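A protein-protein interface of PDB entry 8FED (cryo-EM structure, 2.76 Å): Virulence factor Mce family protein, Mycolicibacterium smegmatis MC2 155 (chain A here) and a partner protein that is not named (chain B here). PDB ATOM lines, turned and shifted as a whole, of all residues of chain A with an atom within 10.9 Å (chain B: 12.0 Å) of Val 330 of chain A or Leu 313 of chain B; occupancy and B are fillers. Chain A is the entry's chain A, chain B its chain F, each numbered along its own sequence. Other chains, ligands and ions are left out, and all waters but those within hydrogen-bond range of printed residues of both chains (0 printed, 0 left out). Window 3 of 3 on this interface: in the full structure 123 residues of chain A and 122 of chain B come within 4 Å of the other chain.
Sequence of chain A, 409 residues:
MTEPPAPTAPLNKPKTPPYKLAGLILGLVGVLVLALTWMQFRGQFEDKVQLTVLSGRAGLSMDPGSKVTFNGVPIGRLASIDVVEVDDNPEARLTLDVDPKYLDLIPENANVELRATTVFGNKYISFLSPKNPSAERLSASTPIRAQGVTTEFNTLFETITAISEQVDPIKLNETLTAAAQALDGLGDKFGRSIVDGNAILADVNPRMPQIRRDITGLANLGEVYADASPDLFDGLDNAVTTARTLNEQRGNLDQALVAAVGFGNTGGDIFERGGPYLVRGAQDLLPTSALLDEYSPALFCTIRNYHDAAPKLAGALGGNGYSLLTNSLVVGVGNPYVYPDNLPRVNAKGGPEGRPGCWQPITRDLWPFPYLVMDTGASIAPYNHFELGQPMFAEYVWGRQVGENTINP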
ATOM      1  N   THR A 326      -7.695 -35.887  27.169  1.00  0.00           N
ATOM      2  CA  THR A 326      -6.529 -35.166  26.685  1.00  0.00           C
ATOM      3  C   THR A 326      -5.496 -36.154  26.163  1.00  0.00           C
ATOM      4  O   THR A 326      -5.439 -37.305  26.601  1.00  0.00           O
ATOM      5  CB  THR A 326      -5.895 -34.295  27.780  1.00  0.00           C
ATOM      6  OG1 THR A 326      -5.779 -35.055  28.988  1.00  0.00           O
ATOM      7  CG2 THR A 326      -6.730 -33.049  28.040  1.00  0.00           C
ATOM      8  N   ASN A 327      -4.679 -35.688  25.221  1.00  0.00           N
ATOM      9  CA  ASN A 327      -3.593 -36.471  24.642  1.00  0.00           C
ATOM     10  C   ASN A 327      -2.284 -35.880  25.152  1.00  0.00           C
ATOM     11  O   ASN A 327      -1.930 -34.750  24.799  1.00  0.00           O
ATOM     12  CB  ASN A 327      -3.658 -36.450  23.117  1.00  0.00           C
ATOM     13  CG  ASN A 327      -3.396 -37.807  22.506  1.00  0.00           C
ATOM     14  OD1 ASN A 327      -3.482 -38.831  23.182  1.00  0.00           O
ATOM     15  ND2 ASN A 327      -3.076 -37.824  21.217  1.00  0.00           N
ATOM     16  N   SER A 328      -1.559 -36.643  25.967  1.00  0.00           N
ATOM     17  CA  SER A 328      -0.425 -36.124  26.727  1.00  0.00           C
ATOM     18  C   SER A 328       0.880 -36.636  26.131  1.00  0.00           C
ATOM     19  O   SER A 328       1.217 -37.815  26.282  1.00  0.00           O
ATOM     20  CB  SER A 328      -0.545 -36.518  28.196  1.00  0.00           C
ATOM     21  OG  SER A 328      -1.769 -36.064  28.745  1.00  0.00           O
ATOM     22  N   LEU A 329       1.626 -35.745  25.481  1.00  0.00           N
ATOM     23  CA  LEU A 329       2.953 -36.051  24.968  1.00  0.00           C
ATOM     24  C   LEU A 329       3.946 -35.029  25.499  1.00  0.00           C
ATOM     25  O   LEU A 329       3.652 -33.832  25.546  1.00  0.00           O
ATOM     26  CB  LEU A 329       2.964 -36.068  23.430  1.00  0.00           C
ATOM     27  CG  LEU A 329       2.462 -34.835  22.672  1.00  0.00           C
ATOM     28  CD1 LEU A 329       3.603 -33.904  22.289  1.00  0.00           C
ATOM     29  CD2 LEU A 329       1.666 -35.244  21.442  1.00  0.00           C
ATOM     30  N   VAL A 330       5.119 -35.506  25.908  1.00  0.00           N
ATOM     31  CA  VAL A 330       6.125 -34.636  26.506  1.00  0.00           C
ATOM     32  C   VAL A 330       6.847 -33.860  25.413  1.00  0.00           C
ATOM     33  O   VAL A 330       7.058 -34.353  24.300  1.00  0.00           O
ATOM     34  CB  VAL A 330       7.102 -35.450  27.377  1.00  0.00           C
ATOM     35  CG1 VAL A 330       6.357 -36.118  28.520  1.00  0.00           C
ATOM     36  CG2 VAL A 330       7.830 -36.490  26.543  1.00  0.00           C
ATOM     37  N   VAL A 331       7.210 -32.616  25.725  1.00  0.00           N
ATOM     38  CA  VAL A 331       7.847 -31.711  24.776  1.00  0.00           C
ATOM     39  C   VAL A 331       8.734 -30.749  25.562  1.00  0.00           C
ATOM     40  O   VAL A 331       8.704 -30.709  26.793  1.00  0.00           O
ATOM     41  CB  VAL A 331       6.797 -30.945  23.934  1.00  0.00           C
ATOM     42  CG1 VAL A 331       6.229 -29.770  24.714  1.00  0.00           C
ATOM     43  CG2 VAL A 331       7.367 -30.510  22.588  1.00  0.00           C
ATOM     44  N   GLY A 332       9.547 -29.978  24.843  1.00  0.00           N
ATOM     45  CA  GLY A 332      10.371 -28.958  25.462  1.00  0.00           C
ATOM     46  C   GLY A 332       9.703 -27.594  25.438  1.00  0.00           C
ATOM     47  O   GLY A 332       8.866 -27.306  24.588  1.00  0.00           O
ATOM     48  N   VAL A 333      10.088 -26.747  26.392  1.00  0.00           N
ATOM     49  CA  VAL A 333       9.473 -25.438  26.559  1.00  0.00           C
ATOM     50  C   VAL A 333      10.523 -24.356  26.348  1.00  0.00           C
ATOM     51  O   VAL A 333      11.724 -24.574  26.519  1.00  0.00           O
ATOM     52  CB  VAL A 333       8.813 -25.282  27.940  1.00  0.00           C
ATOM     53  CG1 VAL A 333       7.525 -26.065  27.990  1.00  0.00           C
ATOM     54  CG2 VAL A 333       9.761 -25.744  29.031  1.00  0.00           C
ATOM     55  N   GLY A 334      10.045 -23.168  25.983  1.00  0.00           N
ATOM     56  CA  GLY A 334      10.920 -22.065  25.660  1.00  0.00           C
ATOM     57  C   GLY A 334      11.368 -21.285  26.879  1.00  0.00           C
ATOM     58  O   GLY A 334      10.990 -21.560  28.017  1.00  0.00           O
ATOM     59  N   ASN A 335      12.201 -20.284  26.618  1.00  0.00           N
ATOM     60  CA  ASN A 335      12.741 -19.460  27.687  1.00  0.00           C
ATOM     61  C   ASN A 335      11.643 -18.586  28.290  1.00  0.00           C
ATOM     62  O   ASN A 335      10.828 -18.019  27.554  1.00  0.00           O
ATOM     63  CB  ASN A 335      13.873 -18.579  27.166  1.00  0.00           C
ATOM     64  CG  ASN A 335      14.848 -19.339  26.299  1.00  0.00           C
ATOM     65  OD1 ASN A 335      15.151 -18.929  25.180  1.00  0.00           O
ATOM     66  ND2 ASN A 335      15.345 -20.459  26.810  1.00  0.00           N
ATOM     67  N   PRO A 336      11.593 -18.462  29.617  1.00  0.00           N
ATOM     68  CA  PRO A 336      10.639 -17.537  30.237  1.00  0.00           C
ATOM     69  C   PRO A 336      10.882 -16.103  29.791  1.00  0.00           C
ATOM     70  O   PRO A 336      11.946 -15.752  29.274  1.00  0.00           O
ATOM     71  CB  PRO A 336      10.906 -17.705  31.737  1.00  0.00           C
ATOM     72  CG  PRO A 336      11.490 -19.066  31.861  1.00  0.00           C
ATOM     73  CD  PRO A 336      12.306 -19.271  30.618  1.00  0.00           C
ATOM     74  N   PHE A 386      15.986 -26.606  17.496  1.00  0.00           N
ATOM     75  CA  PHE A 386      16.192 -27.232  18.797  1.00  0.00           C
ATOM     76  C   PHE A 386      17.456 -26.647  19.416  1.00  0.00           C
ATOM     77  O   PHE A 386      18.562 -26.873  18.916  1.00  0.00           O
ATOM     78  CB  PHE A 386      16.296 -28.749  18.649  1.00  0.00           C
ATOM     79  CG  PHE A 386      16.715 -29.465  19.906  1.00  0.00           C
ATOM     80  CD1 PHE A 386      15.769 -29.890  20.820  1.00  0.00           C
ATOM     81  CD2 PHE A 386      18.051 -29.743  20.156  1.00  0.00           C
ATOM     82  CE1 PHE A 386      16.147 -30.556  21.970  1.00  0.00           C
ATOM     83  CE2 PHE A 386      18.434 -30.405  21.305  1.00  0.00           C
ATOM     84  CZ  PHE A 386      17.482 -30.813  22.211  1.00  0.00           C
ATOM     85  N   GLU A 387      17.292 -25.892  20.499  1.00  0.00           N
ATOM     86  CA  GLU A 387      18.413 -25.315  21.221  1.00  0.00           C
ATOM     87  C   GLU A 387      18.242 -25.551  22.712  1.00  0.00           C
ATOM     88  O   GLU A 387      17.120 -25.635  23.219  1.00  0.00           O
ATOM     89  CB  GLU A 387      18.556 -23.816  20.952  1.00  0.00           C
ATOM     90  CG  GLU A 387      19.104 -23.495  19.579  1.00  0.00           C
ATOM     91  CD  GLU A 387      19.636 -22.085  19.481  1.00  0.00           C
ATOM     92  OE1 GLU A 387      19.857 -21.456  20.537  1.00  0.00           O
ATOM     93  OE2 GLU A 387      19.833 -21.607  18.348  1.00  0.00           O
ATOM     94  N   LEU A 388      19.371 -25.669  23.404  1.00  0.00           N
ATOM     95  CA  LEU A 388      19.349 -25.810  24.850  1.00  0.00           C
ATOM     96  C   LEU A 388      18.848 -24.527  25.503  1.00  0.00           C
ATOM     97  O   LEU A 388      19.122 -23.421  25.029  1.00  0.00           O
ATOM     98  CB  LEU A 388      20.742 -26.175  25.362  1.00  0.00           C
ATOM     99  CG  LEU A 388      21.940 -25.684  24.543  1.00  0.00           C
ATOM    100  CD1 LEU A 388      22.270 -24.226  24.830  1.00  0.00           C
ATOM    101  CD2 LEU A 388      23.154 -26.570  24.784  1.00  0.00           C
ATOM    102  N   GLY A 389      18.087 -24.685  26.583  1.00  0.00           N
ATOM    103  CA  GLY A 389      17.509 -23.558  27.288  1.00  0.00           C
ATOM    104  C   GLY A 389      18.532 -22.586  27.837  1.00  0.00           C
ATOM    105  O   GLY A 389      19.523 -23.004  28.443  1.00  0.00           O
ATOM    106  N   PRO A 391      18.273 -20.359  30.428  1.00  0.00           N
ATOM    107  CA  PRO A 391      18.456 -20.662  31.866  1.00  0.00           C
ATOM    108  C   PRO A 391      18.431 -22.168  32.114  1.00  0.00           C
ATOM    109  O   PRO A 391      17.499 -22.722  32.710  1.00  0.00           O
ATOM    110  CB  PRO A 391      17.270 -19.938  32.516  1.00  0.00           C
ATOM    111  CG  PRO A 391      16.575 -19.178  31.414  1.00  0.00           C
ATOM    112  CD  PRO A 391      16.896 -19.914  30.170  1.00  0.00           C
ATOM    113  N   MET A 392      19.470 -22.850  31.625  1.00  0.00           N
ATOM    114  CA  MET A 392      19.512 -24.309  31.695  1.00  0.00           C
ATOM    115  C   MET A 392      19.508 -24.796  33.139  1.00  0.00           C
ATOM    116  O   MET A 392      18.777 -25.727  33.490  1.00  0.00           O
ATOM    117  CB  MET A 392      20.747 -24.828  30.958  1.00  0.00           C
ATOM    118  CG  MET A 392      20.875 -26.340  30.950  1.00  0.00           C
ATOM    119  SD  MET A 392      22.435 -26.888  30.238  1.00  0.00           S
ATOM    120  CE  MET A 392      22.374 -26.076  28.646  1.00  0.00           C
ATOM    121  N   TYR A 396      17.884 -21.236  43.359  1.00  0.00           N
ATOM    122  CA  TYR A 396      16.899 -20.384  44.009  1.00  0.00           C
ATOM    123  C   TYR A 396      17.307 -20.003  45.427  1.00  0.00           C
ATOM    124  O   TYR A 396      16.451 -19.619  46.231  1.00  0.00           O
ATOM    125  CB  TYR A 396      15.531 -21.068  44.011  1.00  0.00           C
ATOM    126  CG  TYR A 396      15.004 -21.360  42.625  1.00  0.00           C
ATOM    127  CD1 TYR A 396      15.321 -20.532  41.554  1.00  0.00           C
ATOM    128  CD2 TYR A 396      14.211 -22.471  42.381  1.00  0.00           C
ATOM    129  CE1 TYR A 396      14.851 -20.794  40.283  1.00  0.00           C
ATOM    130  CE2 TYR A 396      13.738 -22.743  41.111  1.00  0.00           C
ATOM    131  CZ  TYR A 396      14.061 -21.900  40.067  1.00  0.00           C
ATOM    132  OH  TYR A 396      13.593 -22.163  38.801  1.00  0.00           O
ATOM    133  N   GLY B 307      -8.576 -33.864  23.100  1.00  0.00           N
ATOM    134  CA  GLY B 307      -7.841 -32.653  22.822  1.00  0.00           C
ATOM    135  C   GLY B 307      -6.364 -32.831  23.116  1.00  0.00           C
ATOM    136  O   GLY B 307      -5.965 -33.688  23.898  1.00  0.00           O
ATOM    137  N   LEU B 308      -5.544 -32.006  22.470  1.00  0.00           N
ATOM    138  CA  LEU B 308      -4.096 -32.111  22.594  1.00  0.00           C
ATOM    139  C   LEU B 308      -3.622 -31.273  23.776  1.00  0.00           C
ATOM    140  O   LEU B 308      -3.861 -30.062  23.822  1.00  0.00           O
ATOM    141  CB  LEU B 308      -3.416 -31.662  21.303  1.00  0.00           C
ATOM    142  CG  LEU B 308      -3.785 -32.462  20.054  1.00  0.00           C
ATOM    143  CD1 LEU B 308      -3.074 -31.908  18.831  1.00  0.00           C
ATOM    144  CD2 LEU B 308      -3.454 -33.930  20.249  1.00  0.00           C
ATOM    145  N   LEU B 309      -2.944 -31.921  24.723  1.00  0.00           N
ATOM    146  CA  LEU B 309      -2.451 -31.269  25.936  1.00  0.00           C
ATOM    147  C   LEU B 309      -1.047 -31.798  26.207  1.00  0.00           C
ATOM    148  O   LEU B 309      -0.888 -32.918  26.699  1.00  0.00           O
ATOM    149  CB  LEU B 309      -3.376 -31.529  27.119  1.00  0.00           C
ATOM    150  CG  LEU B 309      -2.953 -30.898  28.446  1.00  0.00           C
ATOM    151  CD1 LEU B 309      -3.448 -29.465  28.540  1.00  0.00           C
ATOM    152  CD2 LEU B 309      -3.448 -31.723  29.621  1.00  0.00           C
ATOM    153  N   HIS B 310      -0.038 -30.994  25.903  1.00  0.00           N
ATOM    154  CA  HIS B 310       1.344 -31.413  26.072  1.00  0.00           C
ATOM    155  C   HIS B 310       1.863 -31.023  27.450  1.00  0.00           C
ATOM    156  O   HIS B 310       1.352 -30.109  28.099  1.00  0.00           O
ATOM    157  CB  HIS B 310       2.230 -30.797  24.992  1.00  0.00           C
ATOM    158  CG  HIS B 310       1.704 -30.980  23.603  1.00  0.00           C
ATOM    159  ND1 HIS B 310       0.805 -31.970  23.271  1.00  0.00           N
ATOM    160  CD2 HIS B 310       1.950 -30.297  22.461  1.00  0.00           C
ATOM    161  CE1 HIS B 310       0.520 -31.889  21.984  1.00  0.00           C
ATOM    162  NE2 HIS B 310       1.202 -30.881  21.469  1.00  0.00           N
ATOM    163  N   PHE B 311       2.898 -31.732  27.891  1.00  0.00           N
ATOM    164  CA  PHE B 311       3.567 -31.451  29.156  1.00  0.00           C
ATOM    165  C   PHE B 311       5.011 -31.078  28.863  1.00  0.00           C
ATOM    166  O   PHE B 311       5.735 -31.845  28.222  1.00  0.00           O
ATOM    167  CB  PHE B 311       3.499 -32.651  30.100  1.00  0.00           C
ATOM    168  CG  PHE B 311       2.125 -32.928  30.634  1.00  0.00           C
ATOM    169  CD1 PHE B 311       1.166 -31.931  30.667  1.00  0.00           C
ATOM    170  CD2 PHE B 311       1.791 -34.184  31.107  1.00  0.00           C
ATOM    171  CE1 PHE B 311      -0.100 -32.181  31.158  1.00  0.00           C
ATOM    172  CE2 PHE B 311       0.527 -34.440  31.598  1.00  0.00           C
ATOM    173  CZ  PHE B 311      -0.419 -33.436  31.624  1.00  0.00           C
ATOM    174  N   GLY B 312       5.425 -29.906  29.337  1.00  0.00           N
ATOM    175  CA  GLY B 312       6.776 -29.440  29.082  1.00  0.00           C
ATOM    176  C   GLY B 312       7.795 -30.132  29.973  1.00  0.00           C
ATOM    177  O   GLY B 312       7.534 -30.438  31.136  1.00  0.00           O
ATOM    178  N   LEU B 313       8.970 -30.382  29.406  1.00  0.00           N
ATOM    179  CA  LEU B 313      10.057 -30.988  30.158  1.00  0.00           C
ATOM    180  C   LEU B 313      10.804 -29.930  30.962  1.00  0.00           C
ATOM    181  O   LEU B 313      10.846 -28.752  30.596  1.00  0.00           O
ATOM    182  CB  LEU B 313      11.022 -31.716  29.223  1.00  0.00           C
ATOM    183  CG  LEU B 313      10.492 -32.990  28.564  1.00  0.00           C
ATOM    184  CD1 LEU B 313      11.571 -33.646  27.721  1.00  0.00           C
ATOM    185  CD2 LEU B 313       9.969 -33.959  29.612  1.00  0.00           C
ATOM    186  N   GLY B 314      11.399 -30.368  32.068  1.00  0.00           N
ATOM    187  CA  GLY B 314      12.101 -29.466  32.959  1.00  0.00           C
ATOM    188  C   GLY B 314      11.288 -29.109  34.185  1.00  0.00           C
ATOM    189  O   GLY B 314      10.233 -28.478  34.074  1.00  0.00           O
ATOM    190  N   ILE B 315      11.770 -29.503  35.361  1.00  0.00           N
ATOM    191  CA  ILE B 315      11.049 -29.317  36.614  1.00  0.00           C
ATOM    192  C   ILE B 315      11.579 -28.072  37.309  1.00  0.00           C
ATOM    193  O   ILE B 315      12.796 -27.855  37.372  1.00  0.00           O
ATOM    194  CB  ILE B 315      11.168 -30.555  37.518  1.00  0.00           C
ATOM    195  CG1 ILE B 315      12.632 -30.973  37.685  1.00  0.00           C
ATOM    196  CG2 ILE B 315      10.344 -31.703  36.956  1.00  0.00           C
ATOM    197  CD1 ILE B 315      12.834 -32.112  38.660  1.00  0.00           C
ATOM    198  N   ASN B 316      10.660 -27.241  37.809  1.00  0.00           N
ATOM    199  CA  ASN B 316      10.982 -26.023  38.557  1.00  0.00           C
ATOM    200  C   ASN B 316      11.850 -25.057  37.756  1.00  0.00           C
ATOM    201  O   ASN B 316      12.692 -24.358  38.323  1.00  0.00           O
ATOM    202  CB  ASN B 316      11.659 -26.349  39.893  1.00  0.00           C
ATOM    203  CG  ASN B 316      10.695 -26.904  40.915  1.00  0.00           C
ATOM    204  OD1 ASN B 316       9.518 -26.548  40.931  1.00  0.00           O
ATOM    205  ND2 ASN B 316      11.189 -27.783  41.776  1.00  0.00           N
ATOM    206  N   ALA B 317      11.665 -24.997  36.430  1.00  0.00           N
ATOM    207  CA  ALA B 317      12.389 -23.987  35.659  1.00  0.00           C
ATOM    208  C   ALA B 317      11.803 -22.600  35.906  1.00  0.00           C
ATOM    209  O   ALA B 317      12.556 -21.699  36.316  1.00  0.00           O
ATOM    210  CB  ALA B 317      12.466 -24.394  34.182  1.00  0.00           C
ATOM    211  N   PRO B 318      10.510 -22.343  35.686  1.00  0.00           N
ATOM    212  CA  PRO B 318       9.872 -21.234  36.398  1.00  0.00           C
ATOM    213  C   PRO B 318       9.196 -21.734  37.661  1.00  0.00           C
ATOM    214  O   PRO B 318       8.379 -22.665  37.613  1.00  0.00           O
ATOM    215  CB  PRO B 318       8.845 -20.700  35.385  1.00  0.00           C
ATOM    216  CG  PRO B 318       8.803 -21.715  34.260  1.00  0.00           C
ATOM    217  CD  PRO B 318       9.553 -22.918  34.724  1.00  0.00           C
ATOM    218  N   PRO B 319       9.499 -21.147  38.813  1.00  0.00           N
ATOM    219  CA  PRO B 319       8.828 -21.558  40.045  1.00  0.00           C
ATOM    220  C   PRO B 319       7.516 -20.817  40.223  1.00  0.00           C
ATOM    221  O   PRO B 319       7.393 -19.648  39.826  1.00  0.00           O
ATOM    222  CB  PRO B 319       9.837 -21.178  41.135  1.00  0.00           C
ATOM    223  CG  PRO B 319      10.553 -20.008  40.565  1.00  0.00           C
ATOM    224  CD  PRO B 319      10.608 -20.214  39.070  1.00  0.00           C
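Of chain B, only Phe 311 and Leu 313 come within 4 Å of Val 330 of chain A. Printed residues of chain B within 4 Å of Leu 329 of chain A: Leu 309 (3.97 Å), His 310 (3.4 Å) and Phe 311 (3.2 Å). Val 331 of chain A touches just these residues of chain B: Phe 311, Gly 312 and Leu 313. No residue of chain B comes within 4 Å of Gly 332 of chain A. Gly 312 of chain B touches two residues of chain A. No residue of chain A comes within 4 Å of Gly 314 of chain B. Of the printed residues of chain B, Tyr 396 of chain A touches Asn 316 (2.4 Å), Ala 317 (2.7 Å) and Pro 319 (3.6 Å). Printed residues of chain B within 4 Å of Ser 328 of chain A: Leu 309 (3.2 Å). Of the printed residues of chain A, Leu 309 of chain B touches Thr 326 (3.8 Å), Asn 327 (2.8 Å), Ser 328 (3.2 Å) and Leu 329 (3.97 Å). Of the printed residues of chain A, His 310 of chain B touches Leu 329 (3.4 Å). Phe 386 of chain A touches none of the printed residues of chain B. Pro 391 of chain A touches none of the printed residues of chain B. The nearest residue of chain A that does not touch Leu 313 of chain B is Gly 332 of chain A (4.4 Å). The nearest printed residue of chain A that does not touch Leu 309 of chain B is Val 330 of chain A (6.6 Å).
Among the printed residues, pairs that only touch across the chains: Thr 326 of chain A with Gly 307 of chain B (3.2 Å), Thr 326 of chain A with Leu 309 of chain B (3.8 Å), Asn 327 of chain A with Leu 308 of chain B (3.8 Å), Ser 328 of chain A with Leu 309 of chain B (3.2 Å), Leu 329 of chain A with Leu 309 of chain B (3.97 Å), Leu 329 of chain A with His 310 of chain B (3.4 Å), Val 330 of chain A with Phe 311 of chain B (3.3 Å), Val 330 of chain A with Leu 313 of chain B (3.9 Å), Val 331 of chain A with Gly 312 of chain B (3.3 Å), Val 333 of chain A with Gly 312 of chain B (3.6 Å), Val 333 of chain A with Leu 313 of chain B (3.6 Å) and Tyr 396 of chain A with Pro 319 of chain B (3.6 Å).
Hydrophobic or aromatic side chains of chain B that line the printed part of chain A: Leu 308, Leu 309, His 310, Leu 313 and Pro 319. Of the 18 printed residues of chain A, 8 touch a printed residue of chain B. Hydrophobic or aromatic side chains of chain A that line the printed part of chain B: Leu 329, Val 330, Val 333 and Tyr 396. Among the printed residues, no Asp or Glu carboxylate lies within 4 Å of a Lys or Arg side-chain nitrogen of the other chain.
The backbone NH (N) of Asn 327 of chain A is in hydrogen-bond range of the backbone carbonyl oxygen (O) of Gly 307 of chain B (2.7 Å). N of Leu 309 of chain B sits at hydrogen-bond distance from O of Asn 327 of chain A (3.0 Å). N of Phe 311 of chain B lies within hydrogen-bond range of O of Leu 329 of chain A (3.2 Å). The backbone NH (N) of Val 331 of chain A is in hydrogen-bond range of the backbone carbonyl oxygen (O) of Phe 311 of chain B (3.0 Å). O of Val 331 of chain A sits at hydrogen-bond distance from N of Leu 313 of chain B, 2.6 Å away. The side-chain hydroxyl (OH) of Tyr 396 of chain A lies within hydrogen-bond range of the backbone carbonyl oxygen (O) of Asn 316 of chain B (2.4 Å). The backbone carbonyl oxygen (O) of Ala 317 of chain B lies within hydrogen-bond range of the side-chain hydroxyl (OH) of Tyr 396 of chain A, 2.7 Å away.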
